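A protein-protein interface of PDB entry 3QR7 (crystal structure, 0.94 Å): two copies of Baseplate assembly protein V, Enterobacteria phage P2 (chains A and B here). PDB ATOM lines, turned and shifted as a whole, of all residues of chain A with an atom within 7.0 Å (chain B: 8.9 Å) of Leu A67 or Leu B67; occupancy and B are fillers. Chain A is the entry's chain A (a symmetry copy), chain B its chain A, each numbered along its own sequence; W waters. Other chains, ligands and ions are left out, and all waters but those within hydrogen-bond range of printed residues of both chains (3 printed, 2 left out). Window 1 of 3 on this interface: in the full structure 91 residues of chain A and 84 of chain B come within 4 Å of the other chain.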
ATOM      1  N   LEU A  56       7.186  10.424  28.150  1.00  0.00           N
ATOM      2  CA  LEU A  56       6.744  11.529  27.294  1.00  0.00           C
ATOM      3  C   LEU A  56       5.213  11.436  27.281  1.00  0.00           C
ATOM      4  O   LEU A  56       4.615  10.705  26.491  1.00  0.00           O
ATOM      5  CB  LEU A  56       7.370  11.421  25.911  1.00  0.00           C
ATOM      6  CG  LEU A  56       8.891  11.269  25.915  1.00  0.00           C
ATOM      7  CD1 LEU A  56       9.405  11.124  24.488  1.00  0.00           C
ATOM      8  CD2 LEU A  56       9.589  12.411  26.622  1.00  0.00           C
ATOM      9  N   PRO A  59       0.152  14.206  23.685  1.00  0.00           N
ATOM     10  CA  PRO A  59      -0.606  13.627  22.575  1.00  0.00           C
ATOM     11  C   PRO A  59       0.272  13.084  21.469  1.00  0.00           C
ATOM     12  O   PRO A  59      -0.152  12.149  20.787  1.00  0.00           O
ATOM     13  CB  PRO A  59      -1.442  14.820  22.075  1.00  0.00           C
ATOM     14  CG  PRO A  59      -1.655  15.659  23.325  1.00  0.00           C
ATOM     15  CD  PRO A  59      -0.293  15.581  24.006  1.00  0.00           C
ATOM     16  N   GLU A  60       1.451  13.661  21.261  1.00  0.00           N
ATOM     17  CA  GLU A  60       2.248  13.303  20.113  1.00  0.00           C
ATOM     18  C   GLU A  60       3.734  13.548  20.406  1.00  0.00           C
ATOM     19  O   GLU A  60       4.108  14.641  20.794  1.00  0.00           O
ATOM     20  CB  GLU A  60       1.806  14.215  18.953  1.00  0.00           C
ATOM     21  CG  GLU A  60       2.410  13.911  17.637  1.00  0.00           C
ATOM     22  CD  GLU A  60       1.703  14.780  16.616  1.00  0.00           C
ATOM     23  OE1 GLU A  60       2.155  15.856  16.262  1.00  0.00           O
ATOM     24  OE2 GLU A  60       0.608  14.358  16.208  1.00  0.00           O
ATOM     25  N   VAL A  61       4.535  12.507  20.140  1.00  0.00           N
ATOM     26  CA  VAL A  61       5.990  12.587  20.096  1.00  0.00           C
ATOM     27  C   VAL A  61       6.372  12.480  18.626  1.00  0.00           C
ATOM     28  O   VAL A  61       5.964  11.531  17.951  1.00  0.00           O
ATOM     29  CB  VAL A  61       6.644  11.457  20.889  1.00  0.00           C
ATOM     30  CG1 VAL A  61       8.144  11.510  20.749  1.00  0.00           C
ATOM     31  CG2 VAL A  61       6.239  11.495  22.352  1.00  0.00           C
ATOM     32  N   VAL A  62       7.162  13.430  18.149  1.00  0.00           N
ATOM     33  CA  VAL A  62       7.634  13.434  16.759  1.00  0.00           C
ATOM     34  C   VAL A  62       9.139  13.280  16.738  1.00  0.00           C
ATOM     35  O   VAL A  62       9.842  14.117  17.323  1.00  0.00           O
ATOM     36  CB  VAL A  62       7.249  14.713  16.048  1.00  0.00           C
ATOM     37  CG1 VAL A  62       7.824  14.733  14.624  1.00  0.00           C
ATOM     38  CG2 VAL A  62       5.724  14.918  16.039  1.00  0.00           C
ATOM     39  N   CYS A  63       9.629  12.254  16.054  1.00  0.00           N
ATOM     40  CA  CYS A  63      11.038  12.103  15.743  1.00  0.00           C
ATOM     41  C   CYS A  63      11.160  12.434  14.264  1.00  0.00           C
ATOM     42  O   CYS A  63      10.517  11.795  13.428  1.00  0.00           O
ATOM     43  CB  CYS A  63      11.527  10.677  16.002  1.00  0.00           C
ATOM     44  SG  CYS A  63      11.235  10.103  17.686  1.00  0.00           S
ATOM     45  N   ASN A  65      13.527  12.120  12.002  1.00  0.00           N
ATOM     46  CA  ASN A  65      14.317  11.277  11.113  1.00  0.00           C
ATOM     47  C   ASN A  65      14.321   9.850  11.648  1.00  0.00           C
ATOM     48  O   ASN A  65      13.264   9.201  11.637  1.00  0.00           O
ATOM     49  CB  ASN A  65      15.695  11.886  10.879  1.00  0.00           C
ATOM     50  CG  ASN A  65      15.616  13.201  10.200  1.00  0.00           C
ATOM     51  OD1 ASN A  65      15.630  14.249  10.855  1.00  0.00           O
ATOM     52  ND2 ASN A  65      15.516  13.179   8.901  1.00  0.00           N
ATOM     53  N   ARG A  66      15.446   9.352  12.128  1.00  0.00           N
ATOM     54  CA  ARG A  66      15.551   7.965  12.585  1.00  0.00           C
ATOM     55  C   ARG A  66      15.171   7.829  14.024  1.00  0.00           C
ATOM     56  O   ARG A  66      15.514   8.678  14.861  1.00  0.00           O
ATOM     57  CB  ARG A  66      16.999   7.437  12.463  1.00  0.00           C
ATOM     58  CG  ARG A  66      17.612   7.484  11.076  1.00  0.00           C
ATOM     59  CD  ARG A  66      19.033   6.914  11.045  1.00  0.00           C
ATOM     60  NE  ARG A  66      20.066   7.718  11.681  1.00  0.00           N
ATOM     61  CZ  ARG A  66      20.653   8.772  11.125  1.00  0.00           C
ATOM     62  NH1 ARG A  66      20.325   9.132   9.895  1.00  0.00           N
ATOM     63  NH2 ARG A  66      21.589   9.438  11.776  1.00  0.00           N
ATOM     64  N   LEU A  67      14.524   6.703  14.342  1.00  0.00           N
ATOM     65  CA  LEU A  67      14.265   6.242  15.697  1.00  0.00           C
ATOM     66  C   LEU A  67      14.802   4.823  15.795  1.00  0.00           C
ATOM     67  O   LEU A  67      14.450   3.972  14.966  1.00  0.00           O
ATOM     68  CB  LEU A  67      12.777   6.260  15.975  1.00  0.00           C
ATOM     69  CG  LEU A  67      12.313   5.651  17.272  1.00  0.00           C
ATOM     70  CD1 LEU A  67      12.906   6.341  18.474  1.00  0.00           C
ATOM     71  CD2 LEU A  67      10.804   5.687  17.308  1.00  0.00           C
ATOM     72  N   ILE A  68      15.636   4.576  16.782  1.00  0.00           N
ATOM     73  CA  ILE A  68      16.253   3.276  17.044  1.00  0.00           C
ATOM     74  C   ILE A  68      15.794   2.852  18.446  1.00  0.00           C
ATOM     75  O   ILE A  68      15.875   3.650  19.382  1.00  0.00           O
ATOM     76  CB  ILE A  68      17.772   3.388  16.985  1.00  0.00           C
ATOM     77  CG1 ILE A  68      18.236   3.932  15.653  1.00  0.00           C
ATOM     78  CG2 ILE A  68      18.417   2.046  17.349  1.00  0.00           C
ATOM     79  CD1 ILE A  68      19.756   4.127  15.573  1.00  0.00           C
ATOM     80  N   THR A  69      15.369   1.598  18.598  1.00  0.00           N
ATOM     81  CA  THR A  69      15.051   1.077  19.900  1.00  0.00           C
ATOM     82  C   THR A  69      15.491  -0.375  20.021  1.00  0.00           C
ATOM     83  O   THR A  69      15.656  -1.074  19.018  1.00  0.00           O
ATOM     84  CB  THR A  69      13.524   1.212  20.210  1.00  0.00           C
ATOM     85  OG1 THR A  69      13.338   0.926  21.591  1.00  0.00           O
ATOM     86  CG2 THR A  69      12.668   0.319  19.333  1.00  0.00           C
ATOM     87  N   LEU A  72      10.166  -2.829  21.046  1.00  0.00           N
ATOM     88  CA  LEU A  72       9.047  -1.961  20.746  1.00  0.00           C
ATOM     89  C   LEU A  72       7.757  -2.598  21.281  1.00  0.00           C
ATOM     90  O   LEU A  72       7.524  -3.795  21.067  1.00  0.00           O
ATOM     91  CB  LEU A  72       8.941  -1.765  19.247  1.00  0.00           C
ATOM     92  CG  LEU A  72       7.755  -0.978  18.756  1.00  0.00           C
ATOM     93  CD1 LEU A  72       7.835   0.470  19.203  1.00  0.00           C
ATOM     94  CD2 LEU A  72       7.653  -1.092  17.259  1.00  0.00           C
ATOM     95  N   THR A  79       0.260   3.042  11.691  1.00  0.00           N
ATOM     96  CA  THR A  79       0.469   2.999  10.257  1.00  0.00           C
ATOM     97  C   THR A  79       1.974   2.957   9.996  1.00  0.00           C
ATOM     98  O   THR A  79       2.783   3.493  10.763  1.00  0.00           O
ATOM     99  CB  THR A  79      -0.135   4.163   9.506  1.00  0.00           C
ATOM    100  OG1 THR A  79       0.454   5.381   9.935  1.00  0.00           O
ATOM    101  CG2 THR A  79      -1.627   4.238   9.715  1.00  0.00           C
ATOM    102  N   VAL B  54      19.709  12.488  19.891  1.00  0.00           N
ATOM    103  CA  VAL B  54      19.067  12.427  21.190  1.00  0.00           C
ATOM    104  C   VAL B  54      19.079  10.984  21.654  1.00  0.00           C
ATOM    105  O   VAL B  54      18.549  10.118  20.978  1.00  0.00           O
ATOM    106  CB  VAL B  54      17.599  12.938  21.135  1.00  0.00           C
ATOM    107  CG1 VAL B  54      16.916  12.776  22.493  1.00  0.00           C
ATOM    108  CG2 VAL B  54      17.536  14.356  20.633  1.00  0.00           C
ATOM    109  N   LEU B  56      18.071   8.403  24.739  1.00  0.00           N
ATOM    110  CA  LEU B  56      17.277   8.086  25.930  1.00  0.00           C
ATOM    111  C   LEU B  56      17.807   6.732  26.416  1.00  0.00           C
ATOM    112  O   LEU B  56      17.382   5.669  25.962  1.00  0.00           O
ATOM    113  CB  LEU B  56      15.791   8.072  25.597  1.00  0.00           C
ATOM    114  CG  LEU B  56      15.290   9.330  24.888  1.00  0.00           C
ATOM    115  CD1 LEU B  56      13.808   9.190  24.563  1.00  0.00           C
ATOM    116  CD2 LEU B  56      15.546  10.590  25.686  1.00  0.00           C
ATOM    117  N   VAL B  61      11.266   3.857  27.667  1.00  0.00           N
ATOM    118  CA  VAL B  61      10.712   5.121  27.198  1.00  0.00           C
ATOM    119  C   VAL B  61       9.230   4.864  26.958  1.00  0.00           C
ATOM    120  O   VAL B  61       8.877   3.933  26.230  1.00  0.00           O
ATOM    121  CB  VAL B  61      11.378   5.587  25.906  1.00  0.00           C
ATOM    122  CG1 VAL B  61      10.722   6.845  25.394  1.00  0.00           C
ATOM    123  CG2 VAL B  61      12.869   5.798  26.091  1.00  0.00           C
ATOM    124  N   VAL B  62       8.383   5.696  27.545  1.00  0.00           N
ATOM    125  CA  VAL B  62       6.928   5.586  27.372  1.00  0.00           C
ATOM    126  C   VAL B  62       6.410   6.819  26.668  1.00  0.00           C
ATOM    127  O   VAL B  62       6.594   7.933  27.181  1.00  0.00           O
ATOM    128  CB  VAL B  62       6.225   5.433  28.703  1.00  0.00           C
ATOM    129  CG1 VAL B  62       4.702   5.403  28.509  1.00  0.00           C
ATOM    130  CG2 VAL B  62       6.717   4.188  29.463  1.00  0.00           C
ATOM    131  N   CYS B  63       5.748   6.631  25.534  1.00  0.00           N
ATOM    132  CA  CYS B  63       4.993   7.675  24.867  1.00  0.00           C
ATOM    133  C   CYS B  63       3.533   7.343  25.130  1.00  0.00           C
ATOM    134  O   CYS B  63       3.067   6.256  24.778  1.00  0.00           O
ATOM    135  CB  CYS B  63       5.261   7.697  23.362  1.00  0.00           C
ATOM    136  SG  CYS B  63       7.004   7.875  22.937  1.00  0.00           S
ATOM    137  N   THR B  64       2.779   8.243  25.758  1.00  0.00           N
ATOM    138  CA  THR B  64       1.457   7.889  26.224  1.00  0.00           C
ATOM    139  C   THR B  64       0.403   7.842  25.109  1.00  0.00           C
ATOM    140  O   THR B  64      -0.678   7.278  25.366  1.00  0.00           O
ATOM    141  CB  THR B  64       1.008   8.810  27.337  1.00  0.00           C
ATOM    142  OG1 THR B  64       1.049  10.151  26.864  1.00  0.00           O
ATOM    143  CG2 THR B  64       1.867   8.630  28.569  1.00  0.00           C
ATOM    144  N   ASN B  65       0.657   8.428  23.957  1.00  0.00           N
ATOM    145  CA  ASN B  65      -0.324   8.484  22.880  1.00  0.00           C
ATOM    146  C   ASN B  65       0.368   8.192  21.554  1.00  0.00           C
ATOM    147  O   ASN B  65       0.814   7.053  21.347  1.00  0.00           O
ATOM    148  CB  ASN B  65      -1.103   9.795  22.930  1.00  0.00           C
ATOM    149  CG  ASN B  65      -1.887   9.929  24.180  1.00  0.00           C
ATOM    150  OD1 ASN B  65      -1.430  10.549  25.147  1.00  0.00           O
ATOM    151  ND2 ASN B  65      -3.056   9.351  24.199  1.00  0.00           N
ATOM    152  N   ARG B  66       0.493   9.166  20.671  1.00  0.00           N
ATOM    153  CA  ARG B  66       1.073   8.946  19.346  1.00  0.00           C
ATOM    154  C   ARG B  66       2.559   9.109  19.360  1.00  0.00           C
ATOM    155  O   ARG B  66       3.100  10.010  20.019  1.00  0.00           O
ATOM    156  CB  ARG B  66       0.532   9.963  18.315  1.00  0.00           C
ATOM    157  CG  ARG B  66      -0.974   9.991  18.131  1.00  0.00           C
ATOM    158  CD  ARG B  66      -1.414  11.004  17.071  1.00  0.00           C
ATOM    159  NE  ARG B  66      -1.294  12.410  17.431  1.00  0.00           N
ATOM    160  CZ  ARG B  66      -2.158  13.072  18.190  1.00  0.00           C
ATOM    161  NH1 ARG B  66      -3.236  12.457  18.647  1.00  0.00           N
ATOM    162  NH2 ARG B  66      -1.971  14.352  18.457  1.00  0.00           N
ATOM    163  N   LEU B  67       3.234   8.280  18.557  1.00  0.00           N
ATOM    164  CA  LEU B  67       4.645   8.403  18.225  1.00  0.00           C
ATOM    165  C   LEU B  67       4.747   8.409  16.708  1.00  0.00           C
ATOM    166  O   LEU B  67       4.218   7.502  16.051  1.00  0.00           O
ATOM    167  CB  LEU B  67       5.415   7.231  18.798  1.00  0.00           C
ATOM    168  CG  LEU B  67       6.864   7.104  18.405  1.00  0.00           C
ATOM    169  CD1 LEU B  67       7.679   8.302  18.823  1.00  0.00           C
ATOM    170  CD2 LEU B  67       7.415   5.831  19.002  1.00  0.00           C
ATOM    171  N   ILE B  68       5.407   9.409  16.167  1.00  0.00           N
ATOM    172  CA  ILE B  68       5.617   9.587  14.731  1.00  0.00           C
ATOM    173  C   ILE B  68       7.137   9.567  14.508  1.00  0.00           C
ATOM    174  O   ILE B  68       7.867  10.263  15.216  1.00  0.00           O
ATOM    175  CB  ILE B  68       5.022  10.911  14.267  1.00  0.00           C
ATOM    176  CG1 ILE B  68       3.550  11.002  14.599  1.00  0.00           C
ATOM    177  CG2 ILE B  68       5.322  11.136  12.781  1.00  0.00           C
ATOM    178  CD1 ILE B  68       2.923  12.348  14.213  1.00  0.00           C
ATOM    179  N   THR B  69       7.599   8.824  13.503  1.00  0.00           N
ATOM    180  CA  THR B  69       8.989   8.854  13.137  1.00  0.00           C
ATOM    181  C   THR B  69       9.150   8.774  11.626  1.00  0.00           C
ATOM    182  O   THR B  69       8.259   8.299  10.917  1.00  0.00           O
ATOM    183  CB  THR B  69       9.786   7.702  13.832  1.00  0.00           C
ATOM    184  OG1 THR B  69      11.172   7.957  13.635  1.00  0.00           O
ATOM    185  CG2 THR B  69       9.393   6.328  13.325  1.00  0.00           C
ATOM    186  N   GLY B  70      10.307   9.213  11.158  1.00  0.00           N
ATOM    187  CA  GLY B  70      10.690   9.016   9.761  1.00  0.00           C
ATOM    188  C   GLY B  70      10.998   7.564   9.472  1.00  0.00           C
ATOM    189  O   GLY B  70      10.258   6.884   8.774  1.00  0.00           O
ATOM    190  N   THR B  71      12.075   7.065  10.040  1.00  0.00           N
ATOM    191  CA  THR B  71      12.415   5.657   9.943  1.00  0.00           C
ATOM    192  C   THR B  71      12.440   5.040  11.327  1.00  0.00           C
ATOM    193  O   THR B  71      12.602   5.731  12.342  1.00  0.00           O
ATOM    194  CB  THR B  71      13.727   5.403   9.226  1.00  0.00           C
ATOM    195  OG1 THR B  71      14.789   6.002   9.944  1.00  0.00           O
ATOM    196  CG2 THR B  71      13.699   5.904   7.792  1.00  0.00           C
ATOM    197  N   LEU B  72      12.285   3.722  11.338  1.00  0.00           N
ATOM    198  CA  LEU B  72      12.273   2.949  12.561  1.00  0.00           C
ATOM    199  C   LEU B  72      13.304   1.816  12.451  1.00  0.00           C
ATOM    200  O   LEU B  72      13.352   1.121  11.429  1.00  0.00           O
ATOM    201  CB  LEU B  72      10.892   2.366  12.783  1.00  0.00           C
ATOM    202  CG  LEU B  72      10.737   1.435  13.957  1.00  0.00           C
ATOM    203  CD1 LEU B  72      10.923   2.172  15.270  1.00  0.00           C
ATOM    204  CD2 LEU B  72       9.399   0.750  13.890  1.00  0.00           C
ATOM    205  N   GLU B  73      14.043   1.571  13.530  1.00  0.00           N
ATOM    206  CA  GLU B  73      14.915   0.429  13.635  1.00  0.00           C
ATOM    207  C   GLU B  73      14.636  -0.229  14.996  1.00  0.00           C
ATOM    208  O   GLU B  73      14.866   0.394  16.019  1.00  0.00           O
ATOM    209  CB  GLU B  73      16.385   0.861  13.526  1.00  0.00           C
ATOM    210  CG  GLU B  73      17.364  -0.258  13.748  1.00  0.00           C
ATOM    211  CD  GLU B  73      18.841   0.156  13.657  1.00  0.00           C
ATOM    212  OE1 GLU B  73      19.165   1.329  13.316  1.00  0.00           O
ATOM    213  OE2 GLU B  73      19.692  -0.728  13.950  1.00  0.00           O
ATOM    214  N   VAL B  74      14.143  -1.462  14.967  1.00  0.00           N
ATOM    215  CA  VAL B  74      13.888  -2.257  16.169  1.00  0.00           C
ATOM    216  C   VAL B  74      14.949  -3.353  16.221  1.00  0.00           C
ATOM    217  O   VAL B  74      15.065  -4.134  15.257  1.00  0.00           O
ATOM    218  CB  VAL B  74      12.490  -2.875  16.161  1.00  0.00           C
ATOM    219  CG1 VAL B  74      12.270  -3.739  17.388  1.00  0.00           C
ATOM    220  CG2 VAL B  74      11.417  -1.783  16.053  1.00  0.00           C
ATOM    221  N   GLN B  75      15.718  -3.437  17.292  1.00  0.00           N
ATOM    222  CA  GLN B  75      16.865  -4.331  17.356  1.00  0.00           C
ATOM    223  C   GLN B  75      16.603  -5.718  17.918  1.00  0.00           C
ATOM    224  O   GLN B  75      17.308  -6.655  17.546  1.00  0.00           O
ATOM    225  CB  GLN B  75      17.977  -3.674  18.168  1.00  0.00           C
ATOM    226  CG  GLN B  75      18.440  -2.370  17.575  1.00  0.00           C
ATOM    227  CD  GLN B  75      19.272  -1.548  18.523  1.00  0.00           C
ATOM    228  OE1 GLN B  75      19.025  -1.492  19.739  1.00  0.00           O
ATOM    229  NE2 GLN B  75      20.262  -0.883  17.960  1.00  0.00           N
HETATM  230  O   HOH W   1      15.607   4.270  12.139  1.00  0.00           O
HETATM  231  O   HOH W   2      -0.704  16.865  17.236  1.00  0.00           O
HETATM  232  O   HOH W   3      15.233   8.685   9.039  1.00  0.00           O
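Of the printed residues of chain B, Pro A59 touches Asn B65 and Arg B66. Of chain B, only Leu B67 (3.8 Å), Thr B69 (3.3 Å), Thr B71 (2.9 Å), Leu B72 (3.4 Å) and Glu B73 (2.8 Å) come within 4 Å of Leu A67. Printed residues of chain A within 4 Å of Cys B63: Leu A56 and Val A61. Of chain A, only Val A61 (3.4 Å) and Leu A67 (3.8 Å) come within 4 Å of Leu B67. Of the printed residues of chain A, Leu B72 touches Leu A67. The nearest printed residue of chain A that does not touch Ile B68 is Leu A67 (5.8 Å).
Leu A56 touches Cys B63. CB of Asn B65 touches O of Pro A59, at 3.3 Å. Glu A60 touches Ile B68 (CD to CD1, 3.6 Å). CA of Leu B67 touches O of Val A61, at 3.4 Å. Val A62 touches Ile B68 (CA to O, 3.5 Å). OG1 of Thr B71 touches CA of Arg A66, at 3.4 Å. Leu A67 touches Thr B69 (CB to OG1, 3.3 Å). Leu A67 touches Leu B72. Ile A68 touches Glu B73. O of Thr A69 touches CA of Val B74, 3.6 Å away.
Water W3 lies within hydrogen-bond range of the side-chain hydroxyl (OG1) of Thr B71 (2.9 Å), the backbone NH (N) of Arg A66 (3.2 Å) and the backbone carbonyl oxygen (O) of Asn A65 (3.3 Å). Water W1 lies within hydrogen-bond range of OG1 of Thr B71 (2.9 Å), O of Leu A67 (3.1 Å), N of Glu B73 (3.4 Å) and N of Leu B72 (3.5 Å). Water W2 lies within hydrogen-bond range of the side-chain carboxylate (OE2) of Glu A60 (3.0 Å) and the guanidinium group (NH2) of Arg B66 (3.1 Å).
Val A61 touches Ile B68, but with the chains exchanged Ile A68 does not touch Val B61 (7.7 Å). Cys A63 touches Ile B68, but with the chains exchanged Ile A68 does not touch Cys B63 (10.4 Å). Asn A65 touches Thr B69, but with the chains exchanged Thr A69 does not touch Asn B65 (13.8 Å). Leu A67 touches Thr B69, but with the chains exchanged Thr A69 does not touch Leu B67 (7.6 Å). Positions printed for both chains: 56, 61, 62, 63, 65, 66, 67, 68, 69 and 72. Of the 29 pairs that touch across the chains among the printed residues, 1 has its exchanged pair printed and touching as well.
The backbone carbonyl oxygen (O) of Val B62 sits at hydrogen-bond distance from the backbone NH (N) of Leu A56. The backbone NH (N) of Thr B64 is in hydrogen-bond range of the backbone carbonyl oxygen (O) of Leu A56 (3.2 Å). The backbone NH (N) of Arg B66 sits at hydrogen-bond distance from the backbone carbonyl oxygen (O) of Pro A59. OE2 of Glu A60 is in salt-bridge range of NE of Arg B66, 3.0 Å away. The backbone carbonyl oxygen (O) of Arg B66 sits at hydrogen-bond distance from the backbone NH (N) of Val A61 (2.9 Å). The backbone NH of Ile B68 lies within hydrogen-bond range of the backbone carbonyl oxygen of Val A61, at 2.8 Å. The backbone carbonyl oxygen of Ile B68 sits at hydrogen-bond distance from the backbone NH of Cys A63 (2.8 Å). OG1 of Thr B69 sits at hydrogen-bond distance from O of Asn A65. The backbone carbonyl oxygen (O) of Cys A63 is in hydrogen-bond range of the backbone NH (N) of Gly B70 (3.4 Å). N of Gly B70 lies within hydrogen-bond range of O of Asn A65. The backbone NH of Thr B71 is in hydrogen-bond range of the backbone carbonyl oxygen of Asn A65 (2.9 Å). O of Thr B71 lies within hydrogen-bond range of N of Leu A67. O of Leu A67 lies within hydrogen-bond range of N of Glu B73. The backbone carbonyl oxygen (O) of Glu B73 sits at hydrogen-bond distance from the backbone NH (N) of Thr A69, at 2.9 Å. The backbone NH (N) of Gln B75 lies within hydrogen-bond range of the backbone carbonyl oxygen (O) of Thr A69 (2.9 Å).
The side-chain amide oxygen (OD1) of Asn B65 lies within hydrogen-bond range of the side-chain hydroxyl (OG1) of Thr B64 (3.0 Å). OG1 of Thr B69 lies within hydrogen-bond range of O of Thr B71 (2.9 Å).
Of the 17 printed residues of chain B, 14 touch a printed residue of chain A. Among the printed residues, Asp or Glu carboxylates within 4 Å of a Lys or Arg side-chain nitrogen of the other chain: Glu A60 with Arg B66.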
